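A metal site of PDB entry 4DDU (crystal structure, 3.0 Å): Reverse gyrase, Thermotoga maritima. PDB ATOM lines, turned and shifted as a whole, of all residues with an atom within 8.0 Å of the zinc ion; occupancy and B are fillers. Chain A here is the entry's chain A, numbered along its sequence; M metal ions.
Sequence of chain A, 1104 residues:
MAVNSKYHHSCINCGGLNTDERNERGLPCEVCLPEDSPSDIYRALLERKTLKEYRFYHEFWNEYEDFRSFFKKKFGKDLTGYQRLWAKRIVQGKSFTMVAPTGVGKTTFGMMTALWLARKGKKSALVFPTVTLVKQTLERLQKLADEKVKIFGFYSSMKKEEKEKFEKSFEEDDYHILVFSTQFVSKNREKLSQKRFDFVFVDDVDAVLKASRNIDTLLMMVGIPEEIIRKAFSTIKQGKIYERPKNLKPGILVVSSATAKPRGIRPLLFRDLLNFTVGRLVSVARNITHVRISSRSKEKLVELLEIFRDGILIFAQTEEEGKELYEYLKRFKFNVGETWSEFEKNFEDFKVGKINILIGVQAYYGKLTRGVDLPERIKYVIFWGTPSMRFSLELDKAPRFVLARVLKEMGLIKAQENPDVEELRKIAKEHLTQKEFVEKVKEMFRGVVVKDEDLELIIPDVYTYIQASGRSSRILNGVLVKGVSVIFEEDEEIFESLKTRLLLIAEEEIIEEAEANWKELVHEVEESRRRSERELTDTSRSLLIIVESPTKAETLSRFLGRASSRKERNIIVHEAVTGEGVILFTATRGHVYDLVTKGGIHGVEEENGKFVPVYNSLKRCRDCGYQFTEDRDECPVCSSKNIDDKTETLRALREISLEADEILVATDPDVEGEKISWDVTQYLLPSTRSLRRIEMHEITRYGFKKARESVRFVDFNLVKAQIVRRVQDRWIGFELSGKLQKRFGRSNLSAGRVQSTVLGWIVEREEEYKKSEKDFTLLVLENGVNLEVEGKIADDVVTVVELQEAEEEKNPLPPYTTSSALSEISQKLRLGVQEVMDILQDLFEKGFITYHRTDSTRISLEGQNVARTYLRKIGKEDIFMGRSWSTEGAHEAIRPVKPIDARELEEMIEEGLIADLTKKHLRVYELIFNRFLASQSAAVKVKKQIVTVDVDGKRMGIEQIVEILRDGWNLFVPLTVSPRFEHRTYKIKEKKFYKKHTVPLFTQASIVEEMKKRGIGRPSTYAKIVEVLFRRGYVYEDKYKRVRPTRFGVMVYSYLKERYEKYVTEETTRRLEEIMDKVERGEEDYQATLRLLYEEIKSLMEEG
The backbone NH of Tyr 626 sits close to the side-chain sulfur of Cys 624, at 3.6 Å. N of Asp 623 sits close to SG of Cys 621, at 3.4 Å. The backbone carbonyl oxygen of Tyr 626 lies within hydrogen-bond range of the backbone NH of Cys 621 (3.1 Å). N of Cys 635 lies within hydrogen-bond range of O of Ser 640. The side-chain sulfur of Cys 635 sits close to the backbone NH of Val 637 (3.5 Å).
Of the 19 residues printed, 4 come within 4 Å of the zinc ion. The nearest printed residue that does not touch the zinc ion is Gly 625 (4.7 Å).
The zinc ion is bound by SG of Cys 624, at 2.2 Å. The zinc ion is bound by SG of Cys 638, at 2.2 Å. The zinc ion is bound by SG of Cys 621 (2.3 Å). SG of Cys 635 binds the zinc ion (2.3 Å). The zinc ion has four donor atoms within binding distance.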
ATOM      1  N   ARG A 620     -20.665 -17.966 -14.638  1.00  0.00           N
ATOM      2  CA  ARG A 620     -20.752 -18.364 -13.237  1.00  0.00           C
ATOM      3  C   ARG A 620     -19.826 -19.536 -12.980  1.00  0.00           C
ATOM      4  O   ARG A 620     -19.970 -20.596 -13.595  1.00  0.00           O
ATOM      5  CB  ARG A 620     -22.190 -18.729 -12.873  1.00  0.00           C
ATOM      6  CG  ARG A 620     -22.481 -18.641 -11.374  1.00  0.00           C
ATOM      7  CD  ARG A 620     -23.870 -19.164 -11.031  1.00  0.00           C
ATOM      8  NE  ARG A 620     -24.022 -20.573 -11.374  1.00  0.00           N
ATOM      9  CZ  ARG A 620     -23.582 -21.581 -10.627  1.00  0.00           C
ATOM     10  NH1 ARG A 620     -22.960 -21.333  -9.479  1.00  0.00           N
ATOM     11  NH2 ARG A 620     -23.756 -22.833 -11.032  1.00  0.00           N
ATOM     12  N   CYS A 621     -18.876 -19.354 -12.074  1.00  0.00           N
ATOM     13  CA  CYS A 621     -17.998 -20.435 -11.673  1.00  0.00           C
ATOM     14  C   CYS A 621     -18.826 -21.519 -10.987  1.00  0.00           C
ATOM     15  O   CYS A 621     -19.520 -21.259 -10.006  1.00  0.00           O
ATOM     16  CB  CYS A 621     -16.909 -19.926 -10.732  1.00  0.00           C
ATOM     17  SG  CYS A 621     -15.755 -21.192 -10.180  1.00  0.00           S
ATOM     18  N   ARG A 622     -18.752 -22.747 -11.507  1.00  0.00           N
ATOM     19  CA  ARG A 622     -19.529 -23.847 -10.956  1.00  0.00           C
ATOM     20  C   ARG A 622     -18.959 -24.335  -9.625  1.00  0.00           C
ATOM     21  O   ARG A 622     -19.562 -25.171  -8.964  1.00  0.00           O
ATOM     22  CB  ARG A 622     -19.624 -25.003 -11.941  1.00  0.00           C
ATOM     23  CG  ARG A 622     -20.306 -24.654 -13.255  1.00  0.00           C
ATOM     24  CD  ARG A 622     -20.674 -25.914 -14.018  1.00  0.00           C
ATOM     25  NE  ARG A 622     -21.117 -25.632 -15.382  1.00  0.00           N
ATOM     26  CZ  ARG A 622     -20.318 -25.644 -16.439  1.00  0.00           C
ATOM     27  NH1 ARG A 622     -19.022 -25.929 -16.293  1.00  0.00           N
ATOM     28  NH2 ARG A 622     -20.800 -25.372 -17.638  1.00  0.00           N
ATOM     29  N   ASP A 623     -17.795 -23.815  -9.253  1.00  0.00           N
ATOM     30  CA  ASP A 623     -17.146 -24.200  -8.002  1.00  0.00           C
ATOM     31  C   ASP A 623     -17.517 -23.261  -6.852  1.00  0.00           C
ATOM     32  O   ASP A 623     -18.348 -23.587  -6.013  1.00  0.00           O
ATOM     33  CB  ASP A 623     -15.635 -24.266  -8.190  1.00  0.00           C
ATOM     34  CG  ASP A 623     -15.213 -25.352  -9.148  1.00  0.00           C
ATOM     35  OD1 ASP A 623     -16.071 -25.812  -9.931  1.00  0.00           O
ATOM     36  OD2 ASP A 623     -14.017 -25.736  -9.142  1.00  0.00           O
ATOM     37  N   CYS A 624     -16.889 -22.083  -6.831  1.00  0.00           N
ATOM     38  CA  CYS A 624     -17.093 -21.132  -5.735  1.00  0.00           C
ATOM     39  C   CYS A 624     -18.397 -20.353  -5.873  1.00  0.00           C
ATOM     40  O   CYS A 624     -18.991 -19.938  -4.880  1.00  0.00           O
ATOM     41  CB  CYS A 624     -15.899 -20.174  -5.632  1.00  0.00           C
ATOM     42  SG  CYS A 624     -15.675 -19.141  -7.089  1.00  0.00           S
ATOM     43  N   GLY A 625     -18.841 -20.151  -7.108  1.00  0.00           N
ATOM     44  CA  GLY A 625     -20.115 -19.512  -7.363  1.00  0.00           C
ATOM     45  C   GLY A 625     -20.044 -18.053  -7.778  1.00  0.00           C
ATOM     46  O   GLY A 625     -21.072 -17.402  -7.957  1.00  0.00           O
ATOM     47  N   TYR A 626     -18.832 -17.538  -7.927  1.00  0.00           N
ATOM     48  CA  TYR A 626     -18.642 -16.131  -8.279  1.00  0.00           C
ATOM     49  C   TYR A 626     -19.115 -15.826  -9.690  1.00  0.00           C
ATOM     50  O   TYR A 626     -18.845 -16.592 -10.617  1.00  0.00           O
ATOM     51  CB  TYR A 626     -17.177 -15.719  -8.113  1.00  0.00           C
ATOM     52  CG  TYR A 626     -16.920 -14.274  -8.426  1.00  0.00           C
ATOM     53  CD1 TYR A 626     -17.324 -13.270  -7.548  1.00  0.00           C
ATOM     54  CD2 TYR A 626     -16.276 -13.900  -9.599  1.00  0.00           C
ATOM     55  CE1 TYR A 626     -17.090 -11.940  -7.838  1.00  0.00           C
ATOM     56  CE2 TYR A 626     -16.042 -12.570  -9.889  1.00  0.00           C
ATOM     57  CZ  TYR A 626     -16.449 -11.590  -9.009  1.00  0.00           C
ATOM     58  OH  TYR A 626     -16.215 -10.269  -9.304  1.00  0.00           O
ATOM     59  N   GLN A 627     -19.817 -14.712  -9.865  1.00  0.00           N
ATOM     60  CA  GLN A 627     -20.305 -14.320 -11.183  1.00  0.00           C
ATOM     61  C   GLN A 627     -19.502 -13.159 -11.760  1.00  0.00           C
ATOM     62  O   GLN A 627     -18.992 -12.314 -11.017  1.00  0.00           O
ATOM     63  CB  GLN A 627     -21.783 -13.959 -11.141  1.00  0.00           C
ATOM     64  CG  GLN A 627     -22.702 -15.101 -10.778  1.00  0.00           C
ATOM     65  CD  GLN A 627     -24.107 -14.911 -11.305  1.00  0.00           C
ATOM     66  OE1 GLN A 627     -24.299 -14.389 -12.402  1.00  0.00           O
ATOM     67  NE2 GLN A 627     -25.088 -15.338 -10.521  1.00  0.00           N
ATOM     68  N   PHE A 628     -19.402 -13.113 -13.075  1.00  0.00           N
ATOM     69  CA  PHE A 628     -18.651 -12.077 -13.760  1.00  0.00           C
ATOM     70  C   PHE A 628     -19.083 -11.896 -15.210  1.00  0.00           C
ATOM     71  O   PHE A 628     -19.780 -12.741 -15.774  1.00  0.00           O
ATOM     72  CB  PHE A 628     -17.139 -12.343 -13.658  1.00  0.00           C
ATOM     73  CG  PHE A 628     -16.723 -13.725 -14.082  1.00  0.00           C
ATOM     74  CD1 PHE A 628     -16.915 -14.819 -13.253  1.00  0.00           C
ATOM     75  CD2 PHE A 628     -16.105 -13.924 -15.308  1.00  0.00           C
ATOM     76  CE1 PHE A 628     -16.534 -16.088 -13.635  1.00  0.00           C
ATOM     77  CE2 PHE A 628     -15.716 -15.191 -15.694  1.00  0.00           C
ATOM     78  CZ  PHE A 628     -15.931 -16.277 -14.860  1.00  0.00           C
ATOM     79  N   GLU A 634     -10.303 -18.442 -16.710  1.00  0.00           N
ATOM     80  CA  GLU A 634     -10.524 -19.003 -15.394  1.00  0.00           C
ATOM     81  C   GLU A 634     -11.436 -18.102 -14.567  1.00  0.00           C
ATOM     82  O   GLU A 634     -11.845 -17.037 -15.017  1.00  0.00           O
ATOM     83  CB  GLU A 634      -9.200 -19.201 -14.645  1.00  0.00           C
ATOM     84  CG  GLU A 634      -8.204 -20.114 -15.339  1.00  0.00           C
ATOM     85  CD  GLU A 634      -7.405 -19.418 -16.426  1.00  0.00           C
ATOM     86  OE1 GLU A 634      -7.617 -18.196 -16.627  1.00  0.00           O
ATOM     87  OE2 GLU A 634      -6.570 -20.076 -17.076  1.00  0.00           O
ATOM     88  N   CYS A 635     -11.754 -18.555 -13.352  1.00  0.00           N
ATOM     89  CA  CYS A 635     -12.527 -17.757 -12.409  1.00  0.00           C
ATOM     90  C   CYS A 635     -11.641 -16.711 -11.765  1.00  0.00           C
ATOM     91  O   CYS A 635     -10.593 -17.037 -11.197  1.00  0.00           O
ATOM     92  CB  CYS A 635     -13.144 -18.663 -11.343  1.00  0.00           C
ATOM     93  SG  CYS A 635     -14.008 -17.808 -10.021  1.00  0.00           S
ATOM     94  N   PRO A 636     -12.038 -15.427 -11.837  1.00  0.00           N
ATOM     95  CA  PRO A 636     -11.224 -14.327 -11.300  1.00  0.00           C
ATOM     96  C   PRO A 636     -10.978 -14.409  -9.791  1.00  0.00           C
ATOM     97  O   PRO A 636     -10.160 -13.669  -9.257  1.00  0.00           O
ATOM     98  CB  PRO A 636     -12.047 -13.078 -11.652  1.00  0.00           C
ATOM     99  CG  PRO A 636     -13.428 -13.584 -11.870  1.00  0.00           C
ATOM    100  CD  PRO A 636     -13.281 -14.951 -12.445  1.00  0.00           C
ATOM    101  N   VAL A 637     -11.684 -15.311  -9.120  1.00  0.00           N
ATOM    102  CA  VAL A 637     -11.532 -15.472  -7.681  1.00  0.00           C
ATOM    103  C   VAL A 637     -10.735 -16.729  -7.316  1.00  0.00           C
ATOM    104  O   VAL A 637      -9.655 -16.633  -6.750  1.00  0.00           O
ATOM    105  CB  VAL A 637     -12.905 -15.501  -6.966  1.00  0.00           C
ATOM    106  CG1 VAL A 637     -12.721 -15.764  -5.482  1.00  0.00           C
ATOM    107  CG2 VAL A 637     -13.635 -14.191  -7.193  1.00  0.00           C
ATOM    108  N   CYS A 638     -11.273 -17.902  -7.657  1.00  0.00           N
ATOM    109  CA  CYS A 638     -10.632 -19.160  -7.278  1.00  0.00           C
ATOM    110  C   CYS A 638      -9.785 -19.772  -8.398  1.00  0.00           C
ATOM    111  O   CYS A 638      -9.270 -20.872  -8.260  1.00  0.00           O
ATOM    112  CB  CYS A 638     -11.678 -20.170  -6.787  1.00  0.00           C
ATOM    113  SG  CYS A 638     -12.718 -20.853  -8.099  1.00  0.00           S
ATOM    114  N   SER A 639      -9.663 -19.040  -9.508  1.00  0.00           N
ATOM    115  CA  SER A 639      -8.771 -19.423 -10.607  1.00  0.00           C
ATOM    116  C   SER A 639      -9.109 -20.769 -11.250  1.00  0.00           C
ATOM    117  O   SER A 639      -8.219 -21.435 -11.798  1.00  0.00           O
ATOM    118  CB  SER A 639      -7.309 -19.382 -10.170  1.00  0.00           C
ATOM    119  OG  SER A 639      -6.943 -18.078  -9.724  1.00  0.00           O
ATOM    120  N   SER A 640     -10.369 -21.169 -11.194  1.00  0.00           N
ATOM    121  CA  SER A 640     -10.808 -22.435 -11.781  1.00  0.00           C
ATOM    122  C   SER A 640     -11.382 -22.249 -13.185  1.00  0.00           C
ATOM    123  O   SER A 640     -11.999 -21.228 -13.478  1.00  0.00           O
ATOM    124  CB  SER A 640     -11.839 -23.116 -10.884  1.00  0.00           C
ATOM    125  OG  SER A 640     -12.332 -24.307 -11.487  1.00  0.00           O
ATOM    126  N   LYS A 641     -11.187 -23.250 -14.038  1.00  0.00           N
ATOM    127  CA  LYS A 641     -11.645 -23.175 -15.420  1.00  0.00           C
ATOM    128  C   LYS A 641     -13.057 -23.722 -15.586  1.00  0.00           C
ATOM    129  O   LYS A 641     -13.692 -23.517 -16.625  1.00  0.00           O
ATOM    130  CB  LYS A 641     -10.693 -23.938 -16.334  1.00  0.00           C
ATOM    131  CG  LYS A 641      -9.298 -23.355 -16.427  1.00  0.00           C
ATOM    132  CD  LYS A 641      -8.479 -24.062 -17.498  1.00  0.00           C
ATOM    133  CE  LYS A 641      -9.160 -23.974 -18.854  1.00  0.00           C
ATOM    134  NZ  LYS A 641      -8.423 -24.718 -19.902  1.00  0.00           N
ATOM    135  N   ASN A 642     -13.554 -24.424 -14.574  1.00  0.00           N
ATOM    136  CA  ASN A 642     -14.885 -25.023 -14.637  1.00  0.00           C
ATOM    137  C   ASN A 642     -15.984 -23.997 -14.459  1.00  0.00           C
ATOM    138  O   ASN A 642     -16.561 -23.859 -13.371  1.00  0.00           O
ATOM    139  CB  ASN A 642     -15.005 -26.147 -13.598  1.00  0.00           C
ATOM    140  CG  ASN A 642     -16.379 -26.811 -13.627  1.00  0.00           C
ATOM    141  OD1 ASN A 642     -17.093 -26.791 -12.624  1.00  0.00           O
ATOM    142  ND2 ASN A 642     -16.743 -27.377 -14.757  1.00  0.00           N
ATOM    143  N   ILE A 643     -16.286 -23.265 -15.532  1.00  0.00           N
ATOM    144  CA  ILE A 643     -17.312 -22.220 -15.471  1.00  0.00           C
ATOM    145  C   ILE A 643     -18.473 -22.492 -16.413  1.00  0.00           C
ATOM    146  O   ILE A 643     -18.388 -23.309 -17.320  1.00  0.00           O
ATOM    147  CB  ILE A 643     -16.729 -20.827 -15.795  1.00  0.00           C
ATOM    148  CG1 ILE A 643     -16.414 -20.722 -17.290  1.00  0.00           C
ATOM    149  CG2 ILE A 643     -15.501 -20.547 -14.947  1.00  0.00           C
ATOM    150  CD1 ILE A 643     -15.920 -19.359 -17.713  1.00  0.00           C
HETATM  151 ZN    ZN M   1     -14.536 -19.766  -8.846  1.00  0.00          ZN
